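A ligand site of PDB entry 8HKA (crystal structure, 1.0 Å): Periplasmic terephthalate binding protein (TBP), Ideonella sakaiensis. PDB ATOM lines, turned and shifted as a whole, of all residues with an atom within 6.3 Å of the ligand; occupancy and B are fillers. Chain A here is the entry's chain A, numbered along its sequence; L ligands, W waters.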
ATOM      1  N   TYR A  15      18.222  -9.428  -2.973  1.00  0.00           N
ATOM      2  CA  TYR A  15      17.960  -9.704  -4.361  1.00  0.00           C
ATOM      3  C   TYR A  15      18.044  -8.408  -5.139  1.00  0.00           C
ATOM      4  O   TYR A  15      17.897  -7.312  -4.562  1.00  0.00           O
ATOM      5  CB  TYR A  15      16.544 -10.339  -4.530  1.00  0.00           C
ATOM      6  CG  TYR A  15      16.434 -11.702  -3.904  1.00  0.00           C
ATOM      7  CD1 TYR A  15      16.976 -12.821  -4.529  1.00  0.00           C
ATOM      8  CD2 TYR A  15      15.914 -11.840  -2.616  1.00  0.00           C
ATOM      9  CE1 TYR A  15      17.004 -14.034  -3.876  1.00  0.00           C
ATOM     10  CE2 TYR A  15      15.915 -13.047  -1.981  1.00  0.00           C
ATOM     11  CZ  TYR A  15      16.445 -14.148  -2.610  1.00  0.00           C
ATOM     12  OH  TYR A  15      16.403 -15.357  -1.957  1.00  0.00           O
ATOM     13  N   PRO A  16      18.291  -8.486  -6.452  1.00  0.00           N
ATOM     14  CA  PRO A  16      18.410  -7.296  -7.270  1.00  0.00           C
ATOM     15  C   PRO A  16      17.122  -6.454  -7.300  1.00  0.00           C
ATOM     16  O   PRO A  16      15.987  -6.988  -7.221  1.00  0.00           O
ATOM     17  CB  PRO A  16      18.675  -7.815  -8.692  1.00  0.00           C
ATOM     18  CG  PRO A  16      19.079  -9.206  -8.538  1.00  0.00           C
ATOM     19  CD  PRO A  16      18.490  -9.708  -7.240  1.00  0.00           C
ATOM     20  N   GLY A  18      13.962  -4.335  -8.508  1.00  0.00           N
ATOM     21  CA  GLY A  18      13.006  -4.374  -9.577  1.00  0.00           C
ATOM     22  C   GLY A  18      12.142  -5.615  -9.566  1.00  0.00           C
ATOM     23  O   GLY A  18      11.095  -5.602 -10.246  1.00  0.00           O
ATOM     24  N   GLY A  19      12.517  -6.709  -8.885  1.00  0.00           N
ATOM     25  CA  GLY A  19      11.649  -7.849  -8.679  1.00  0.00           C
ATOM     26  C   GLY A  19      10.684  -7.592  -7.534  1.00  0.00           C
ATOM     27  O   GLY A  19      10.703  -6.521  -6.917  1.00  0.00           O
ATOM     28  N   THR A  20       9.846  -8.585  -7.187  1.00  0.00           N
ATOM     29  CA  THR A  20       8.872  -8.391  -6.126  1.00  0.00           C
ATOM     30  C   THR A  20       9.562  -8.202  -4.775  1.00  0.00           C
ATOM     31  O   THR A  20       9.058  -7.526  -3.908  1.00  0.00           O
ATOM     32  CB  THR A  20       7.874  -9.568  -6.147  1.00  0.00           C
ATOM     33  OG1 THR A  20       7.352  -9.611  -7.462  1.00  0.00           O
ATOM     34  CG2 THR A  20       6.787  -9.365  -5.131  1.00  0.00           C
ATOM     35  N   ALA A  21      10.656  -8.908  -4.566  1.00  0.00           N
ATOM     36  CA  ALA A  21      11.352  -8.851  -3.283  1.00  0.00           C
ATOM     37  C   ALA A  21      11.728  -7.392  -2.975  1.00  0.00           C
ATOM     38  O   ALA A  21      11.677  -6.961  -1.831  1.00  0.00           O
ATOM     39  CB  ALA A  21      12.610  -9.682  -3.293  1.00  0.00           C
ATOM     40  N   ASP A  22      12.104  -6.654  -3.997  1.00  0.00           N
ATOM     41  CA  ASP A  22      12.485  -5.251  -3.885  1.00  0.00           C
ATOM     42  C   ASP A  22      11.279  -4.322  -3.862  1.00  0.00           C
ATOM     43  O   ASP A  22      11.215  -3.380  -3.068  1.00  0.00           O
ATOM     44  CB  ASP A  22      13.416  -4.906  -5.034  1.00  0.00           C
ATOM     45  CG  ASP A  22      13.827  -3.475  -5.081  1.00  0.00           C
ATOM     46  OD1 ASP A  22      14.581  -3.052  -4.186  1.00  0.00           O
ATOM     47  OD2 ASP A  22      13.389  -2.789  -6.043  1.00  0.00           O
ATOM     48  N   PRO A  71      12.010 -12.894   0.405  1.00  0.00           N
ATOM     49  CA  PRO A  71      11.279 -14.118   0.100  1.00  0.00           C
ATOM     50  C   PRO A  71      11.956 -15.306   0.791  1.00  0.00           C
ATOM     51  O   PRO A  71      12.927 -15.158   1.591  1.00  0.00           O
ATOM     52  CB  PRO A  71      11.309 -14.175  -1.435  1.00  0.00           C
ATOM     53  CG  PRO A  71      12.563 -13.386  -1.840  1.00  0.00           C
ATOM     54  CD  PRO A  71      12.657 -12.323  -0.793  1.00  0.00           C
ATOM     55  N   PRO A  72      11.422 -16.514   0.608  1.00  0.00           N
ATOM     56  CA  PRO A  72      11.697 -17.623   1.541  1.00  0.00           C
ATOM     57  C   PRO A  72      13.106 -18.188   1.581  1.00  0.00           C
ATOM     58  O   PRO A  72      13.410 -18.886   2.566  1.00  0.00           O
ATOM     59  CB  PRO A  72      10.708 -18.706   1.135  1.00  0.00           C
ATOM     60  CG  PRO A  72       9.552 -17.935   0.519  1.00  0.00           C
ATOM     61  CD  PRO A  72      10.257 -16.815  -0.236  1.00  0.00           C
ATOM     62  N   GLY A  73      13.890 -18.065   0.529  1.00  0.00           N
ATOM     63  CA  GLY A  73      15.171 -18.750   0.449  1.00  0.00           C
ATOM     64  C   GLY A  73      15.978 -18.707   1.734  1.00  0.00           C
ATOM     65  O   GLY A  73      16.252 -19.738   2.353  1.00  0.00           O
ATOM     66  N   ILE A  77      14.136 -21.924   3.316  1.00  0.00           N
ATOM     67  CA  ILE A  77      14.359 -22.983   2.332  1.00  0.00           C
ATOM     68  C   ILE A  77      15.813 -23.400   2.194  1.00  0.00           C
ATOM     69  O   ILE A  77      16.130 -24.605   2.244  1.00  0.00           O
ATOM     70  CB  ILE A  77      13.786 -22.658   0.941  1.00  0.00           C
ATOM     71  CG1 ILE A  77      12.302 -22.299   1.031  1.00  0.00           C
ATOM     72  CG2 ILE A  77      13.988 -23.836  -0.004  1.00  0.00           C
ATOM     73  CD1 ILE A  77      11.657 -21.974  -0.320  1.00  0.00           C
ATOM     74  N   ASN A 103       3.104 -18.367  -7.347  1.00  0.00           N
ATOM     75  CA  ASN A 103       3.975 -18.552  -8.481  1.00  0.00           C
ATOM     76  C   ASN A 103       3.181 -18.985  -9.722  1.00  0.00           C
ATOM     77  O   ASN A 103       2.018 -19.433  -9.663  1.00  0.00           O
ATOM     78  CB  ASN A 103       5.127 -19.537  -8.206  1.00  0.00           C
ATOM     79  CG  ASN A 103       6.183 -18.989  -7.244  1.00  0.00           C
ATOM     80  OD1 ASN A 103       6.978 -19.785  -6.705  1.00  0.00           O
ATOM     81  ND2 ASN A 103       6.276 -17.707  -7.122  1.00  0.00           N
ATOM     82  N   GLN A 135      15.409 -17.656  -9.740  1.00  0.00           N
ATOM     83  CA  GLN A 135      15.869 -16.541  -8.919  1.00  0.00           C
ATOM     84  C   GLN A 135      17.120 -16.876  -8.107  1.00  0.00           C
ATOM     85  O   GLN A 135      17.561 -16.038  -7.358  1.00  0.00           O
ATOM     86  CB  GLN A 135      14.762 -16.176  -7.923  1.00  0.00           C
ATOM     87  CG  GLN A 135      13.445 -15.760  -8.568  1.00  0.00           C
ATOM     88  CD  GLN A 135      12.218 -16.293  -7.889  1.00  0.00           C
ATOM     89  OE1 GLN A 135      12.255 -17.263  -7.124  1.00  0.00           O
ATOM     90  NE2 GLN A 135      11.091 -15.658  -8.201  1.00  0.00           N
ATOM     91  N   GLY A 138      17.609 -22.667  -4.428  1.00  0.00           N
ATOM     92  CA  GLY A 138      16.842 -22.678  -3.186  1.00  0.00           C
ATOM     93  C   GLY A 138      15.729 -21.624  -3.116  1.00  0.00           C
ATOM     94  O   GLY A 138      14.981 -21.607  -2.151  1.00  0.00           O
ATOM     95  N   THR A 139      15.575 -20.804  -4.164  1.00  0.00           N
ATOM     96  CA  THR A 139      14.445 -19.884  -4.211  1.00  0.00           C
ATOM     97  C   THR A 139      13.174 -20.654  -4.553  1.00  0.00           C
ATOM     98  O   THR A 139      13.219 -21.771  -5.077  1.00  0.00           O
ATOM     99  CB  THR A 139      14.726 -18.766  -5.219  1.00  0.00           C
ATOM    100  OG1 THR A 139      14.799 -19.311  -6.531  1.00  0.00           O
ATOM    101  CG2 THR A 139      15.945 -17.949  -4.852  1.00  0.00           C
ATOM    102  N   THR A 140      12.012 -20.035  -4.363  1.00  0.00           N
ATOM    103  CA  THR A 140      10.819 -20.785  -4.651  1.00  0.00           C
ATOM    104  C   THR A 140      10.703 -21.055  -6.152  1.00  0.00           C
ATOM    105  O   THR A 140      10.125 -22.089  -6.520  1.00  0.00           O
ATOM    106  CB  THR A 140       9.537 -20.144  -4.153  1.00  0.00           C
ATOM    107  OG1 THR A 140       9.192 -18.999  -4.911  1.00  0.00           O
ATOM    108  CG2 THR A 140       9.553 -19.865  -2.662  1.00  0.00           C
ATOM    109  N   SER A 141      11.195 -20.182  -7.028  1.00  0.00           N
ATOM    110  CA  SER A 141      11.121 -20.484  -8.453  1.00  0.00           C
ATOM    111  C   SER A 141      11.883 -21.771  -8.789  1.00  0.00           C
ATOM    112  O   SER A 141      11.470 -22.523  -9.699  1.00  0.00           O
ATOM    113  CB  SER A 141      11.644 -19.325  -9.284  1.00  0.00           C
ATOM    114  OG  SER A 141      13.004 -19.089  -8.986  1.00  0.00           O
ATOM    115  N   LYS A 162      20.526 -14.302 -10.102  1.00  0.00           N
ATOM    116  CA  LYS A 162      20.584 -13.682  -8.763  1.00  0.00           C
ATOM    117  C   LYS A 162      19.228 -13.230  -8.261  1.00  0.00           C
ATOM    118  O   LYS A 162      19.118 -12.793  -7.104  1.00  0.00           O
ATOM    119  CB  LYS A 162      21.616 -12.583  -8.730  1.00  0.00           C
ATOM    120  CG  LYS A 162      23.027 -13.156  -8.637  1.00  0.00           C
ATOM    121  CD  LYS A 162      24.162 -12.121  -8.781  1.00  0.00           C
ATOM    122  CE  LYS A 162      24.424 -11.866 -10.254  1.00  0.00           C
ATOM    123  NZ  LYS A 162      25.285 -10.666 -10.369  1.00  0.00           N
ATOM    124  N   GLY A 163      18.205 -13.219  -9.101  1.00  0.00           N
ATOM    125  CA  GLY A 163      16.845 -12.912  -8.702  1.00  0.00           C
ATOM    126  C   GLY A 163      15.949 -12.848  -9.923  1.00  0.00           C
ATOM    127  O   GLY A 163      16.363 -13.169 -11.033  1.00  0.00           O
ATOM    128  N   THR A 164      14.707 -12.399  -9.679  1.00  0.00           N
ATOM    129  CA  THR A 164      13.738 -12.259 -10.757  1.00  0.00           C
ATOM    130  C   THR A 164      14.226 -11.321 -11.844  1.00  0.00           C
ATOM    131  O   THR A 164      14.030 -11.637 -13.023  1.00  0.00           O
ATOM    132  CB  THR A 164      12.414 -11.754 -10.184  1.00  0.00           C
ATOM    133  OG1 THR A 164      11.747 -12.827  -9.502  1.00  0.00           O
ATOM    134  CG2 THR A 164      11.494 -11.195 -11.257  1.00  0.00           C
ATOM    135  N   ALA A 165      14.782 -10.192 -11.495  1.00  0.00           N
ATOM    136  CA  ALA A 165      14.982  -9.145 -12.494  1.00  0.00           C
ATOM    137  C   ALA A 165      15.877  -9.650 -13.644  1.00  0.00           C
ATOM    138  O   ALA A 165      15.499  -9.538 -14.825  1.00  0.00           O
ATOM    139  CB  ALA A 165      15.470  -7.872 -11.856  1.00  0.00           C
ATOM    140  N   PRO A 166      17.071 -10.234 -13.376  1.00  0.00           N
ATOM    141  CA  PRO A 166      17.904 -10.678 -14.484  1.00  0.00           C
ATOM    142  C   PRO A 166      17.311 -11.885 -15.197  1.00  0.00           C
ATOM    143  O   PRO A 166      17.555 -12.056 -16.404  1.00  0.00           O
ATOM    144  CB  PRO A 166      19.257 -11.001 -13.820  1.00  0.00           C
ATOM    145  CG  PRO A 166      18.906 -11.265 -12.352  1.00  0.00           C
ATOM    146  CD  PRO A 166      17.804 -10.241 -12.102  1.00  0.00           C
ATOM    147  N   ASP A 181       8.282 -17.750 -11.991  1.00  0.00           N
ATOM    148  CA  ASP A 181       8.299 -16.516 -11.222  1.00  0.00           C
ATOM    149  C   ASP A 181       7.041 -16.396 -10.349  1.00  0.00           C
ATOM    150  O   ASP A 181       6.103 -17.188 -10.496  1.00  0.00           O
ATOM    151  CB  ASP A 181       8.377 -15.320 -12.167  1.00  0.00           C
ATOM    152  CG  ASP A 181       8.806 -13.999 -11.558  1.00  0.00           C
ATOM    153  OD1 ASP A 181       9.464 -13.996 -10.483  1.00  0.00           O
ATOM    154  OD2 ASP A 181       8.460 -12.951 -12.188  1.00  0.00           O
ATOM    155  N   ASN A 182       7.015 -15.410  -9.440  1.00  0.00           N
ATOM    156  CA  ASN A 182       5.743 -15.037  -8.859  1.00  0.00           C
ATOM    157  C   ASN A 182       4.929 -14.132  -9.783  1.00  0.00           C
ATOM    158  O   ASN A 182       5.442 -13.461 -10.679  1.00  0.00           O
ATOM    159  CB  ASN A 182       5.893 -14.439  -7.471  1.00  0.00           C
ATOM    160  CG  ASN A 182       6.747 -13.210  -7.432  1.00  0.00           C
ATOM    161  OD1 ASN A 182       7.980 -13.312  -7.164  1.00  0.00           O
ATOM    162  ND2 ASN A 182       6.172 -12.085  -7.725  1.00  0.00           N
ATOM    163  N   SER A 185       5.700  -9.919 -10.279  1.00  0.00           N
ATOM    164  CA  SER A 185       6.728  -9.388 -11.163  1.00  0.00           C
ATOM    165  C   SER A 185       6.441  -9.757 -12.608  1.00  0.00           C
ATOM    166  O   SER A 185       6.886  -9.025 -13.516  1.00  0.00           O
ATOM    167  CB  SER A 185       8.118  -9.769 -10.727  1.00  0.00           C
ATOM    168  OG  SER A 185       8.157 -11.114 -10.317  1.00  0.00           O
ATOM    169  N   THR A 227       4.677 -18.182  -2.901  1.00  0.00           N
ATOM    170  CA  THR A 227       5.777 -17.540  -2.210  1.00  0.00           C
ATOM    171  C   THR A 227       5.239 -16.472  -1.238  1.00  0.00           C
ATOM    172  O   THR A 227       4.040 -16.237  -1.102  1.00  0.00           O
ATOM    173  CB  THR A 227       6.834 -17.034  -3.200  1.00  0.00           C
ATOM    174  OG1 THR A 227       8.011 -16.802  -2.403  1.00  0.00           O
ATOM    175  CG2 THR A 227       6.419 -15.805  -3.960  1.00  0.00           C
ATOM    176  N   TRP A 228       6.197 -15.779  -0.612  1.00  0.00           N
ATOM    177  CA  TRP A 228       5.856 -14.795   0.380  1.00  0.00           C
ATOM    178  C   TRP A 228       7.077 -13.944   0.652  1.00  0.00           C
ATOM    179  O   TRP A 228       8.205 -14.316   0.300  1.00  0.00           O
ATOM    180  CB  TRP A 228       5.288 -15.432   1.665  1.00  0.00           C
ATOM    181  CG  TRP A 228       6.023 -16.634   2.144  1.00  0.00           C
ATOM    182  CD1 TRP A 228       5.618 -17.925   1.897  1.00  0.00           C
ATOM    183  CD2 TRP A 228       7.172 -16.727   3.003  1.00  0.00           C
ATOM    184  NE1 TRP A 228       6.464 -18.817   2.517  1.00  0.00           N
ATOM    185  CE2 TRP A 228       7.405 -18.105   3.231  1.00  0.00           C
ATOM    186  CE3 TRP A 228       8.050 -15.798   3.558  1.00  0.00           C
ATOM    187  CZ2 TRP A 228       8.460 -18.570   4.008  1.00  0.00           C
ATOM    188  CZ3 TRP A 228       9.102 -16.263   4.344  1.00  0.00           C
ATOM    189  CH2 TRP A 228       9.292 -17.640   4.559  1.00  0.00           C
ATOM    190  N   PHE A 229       6.831 -12.816   1.304  1.00  0.00           N
ATOM    191  CA  PHE A 229       7.843 -11.772   1.488  1.00  0.00           C
ATOM    192  C   PHE A 229       7.721 -11.393   2.957  1.00  0.00           C
ATOM    193  O   PHE A 229       6.685 -10.836   3.354  1.00  0.00           O
ATOM    194  CB  PHE A 229       7.548 -10.604   0.537  1.00  0.00           C
ATOM    195  CG  PHE A 229       7.701 -11.051  -0.890  1.00  0.00           C
ATOM    196  CD1 PHE A 229       6.603 -11.568  -1.583  1.00  0.00           C
ATOM    197  CD2 PHE A 229       8.950 -11.042  -1.497  1.00  0.00           C
ATOM    198  CE1 PHE A 229       6.809 -12.123  -2.844  1.00  0.00           C
ATOM    199  CE2 PHE A 229       9.129 -11.583  -2.757  1.00  0.00           C
ATOM    200  CZ  PHE A 229       8.064 -12.132  -3.428  1.00  0.00           C
HETATM  201  C1  LIG L   1      13.143 -14.850  -5.015  1.00  0.00           C
HETATM  202  C2  LIG L   1      13.601 -13.672  -5.563  1.00  0.00           C
HETATM  203  C3  LIG L   1      12.691 -12.640  -5.871  1.00  0.00           C
HETATM  204  C4  LIG L   1      11.329 -12.822  -5.566  1.00  0.00           C
HETATM  205  C5  LIG L   1      10.892 -14.032  -5.031  1.00  0.00           C
HETATM  206  C6  LIG L   1      11.792 -15.055  -4.747  1.00  0.00           C
HETATM  207  C7  LIG L   1      11.283 -16.370  -4.252  1.00  0.00           C
HETATM  208  C8  LIG L   1      13.143 -11.369  -6.497  1.00  0.00           C
HETATM  209  O1  LIG L   1      10.036 -16.596  -4.318  1.00  0.00           O
HETATM  210  O2  LIG L   1      12.086 -17.189  -3.741  1.00  0.00           O
HETATM  211  O3  LIG L   1      14.288 -11.378  -7.072  1.00  0.00           O
HETATM  212  O4  LIG L   1      12.397 -10.354  -6.484  1.00  0.00           O
HETATM  213  O   HOH W   1      13.521  -7.882  -6.237  1.00  0.00           O
HETATM  214  O   HOH W   2       9.786 -11.265  -8.154  1.00  0.00           O
HETATM  215  O   HOH W   3      13.911 -16.657  -1.827  1.00  0.00           O
HETATM  216  O   HOH W   4      15.163  -9.402  -8.737  1.00  0.00           O
HETATM  217  O   HOH W   5       8.685 -16.187  -6.696  1.00  0.00           O
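The backbone NH (N) of Thr 140 lies within hydrogen-bond range of an oxygen (O2) of the ligand, at 2.9 Å. The side-chain hydroxyl (OG1) of Thr 140 lies within hydrogen-bond range of an oxygen (O1) of the ligand, 2.6 Å away. The side-chain hydroxyl of Thr 227 sits at hydrogen-bond distance from an oxygen (O1) of the ligand, 2.8 Å away. The backbone NH (N) of Thr 164 is in hydrogen-bond range of an oxygen (O3) of the ligand (2.8 Å). An oxygen (O4) of the ligand sits at hydrogen-bond distance from the backbone NH (N) of Ala 21 (3.0 Å). OE1 of Gln 135 sits close to O2 of the ligand, at 3.4 Å. The backbone NH (N) of Thr 20 lies within hydrogen-bond range of an oxygen (O4) of the ligand, 3.2 Å away.
OD1 of Asn 103 sits at hydrogen-bond distance from OG1 of Thr 140 (3.0 Å). The side-chain carboxylate (OD1) of Asp 181 lies within hydrogen-bond range of the side-chain hydroxyl (OG1) of Thr 164, 2.7 Å away. The side-chain hydroxyl of Thr 139 is in hydrogen-bond range of the side-chain amide oxygen of Gln 135, 3.3 Å away. NE2 of Gln 135 is in hydrogen-bond range of OD1 of Asp 181 (3.3 Å). OG1 of Thr 20 lies within hydrogen-bond range of ND2 of Asn 182, at 2.8 Å. OG1 of Thr 20 is in hydrogen-bond range of N of Ser 185. OG1 of Thr 139 is in hydrogen-bond range of OG of Ser 141 (3.0 Å). The backbone carbonyl oxygen (O) of Pro 72 lies within hydrogen-bond range of the backbone NH (N) of Ile 77, 3.2 Å away.
Tyr 15 touches the ligand. Gly 19 touches the ligand. Pro 71 touches the ligand (CG to C6, 3.4 Å). CD of Pro 72 touches O2 of the ligand, at 3.97 Å. Thr 139 touches the ligand. Gly 163 touches the ligand (CA to O3, 3.4 Å). OD1 of Asn 182 touches C5 of the ligand (3.7 Å). Phe 229 touches the ligand. Hydrophobic or aromatic side chains that line the ligand: Tyr 15, Ala 21, Pro 71, Pro 72 and Phe 229. 14 residues have an atom within 4 Å of the ligand: Tyr 15, Gly 19, Thr 20, Ala 21, Pro 71, Pro 72, Gln 135, Thr 139, Thr 140, Gly 163, Thr 164, Asn 182, Thr 227 and Phe 229.
Water W3 lies within hydrogen-bond range of an oxygen (O2) of the ligand, the backbone NH (N) of Gly 73 and the side-chain hydroxyl (OH) of Tyr 15. Water W4 lies within hydrogen-bond range of an oxygen (O3) of the ligand, the backbone NH of Ala 165, the backbone carbonyl oxygen of Pro 16 and the backbone NH of Thr 164. Water W5 lies within hydrogen-bond range of O1 of the ligand (2.8 Å), ND2 of Asn 103 (2.9 Å), NE2 of Gln 135 (2.9 Å), OD1 of Asn 182 (3.0 Å) and OG1 of Thr 140 (3.4 Å). Water W2 lies within hydrogen-bond range of the side-chain hydroxyl of Ser 185, the side-chain hydroxyl of Thr 164, the backbone NH of Thr 20, the side-chain amide oxygen of Asn 182 and an oxygen (O4) of the ligand.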
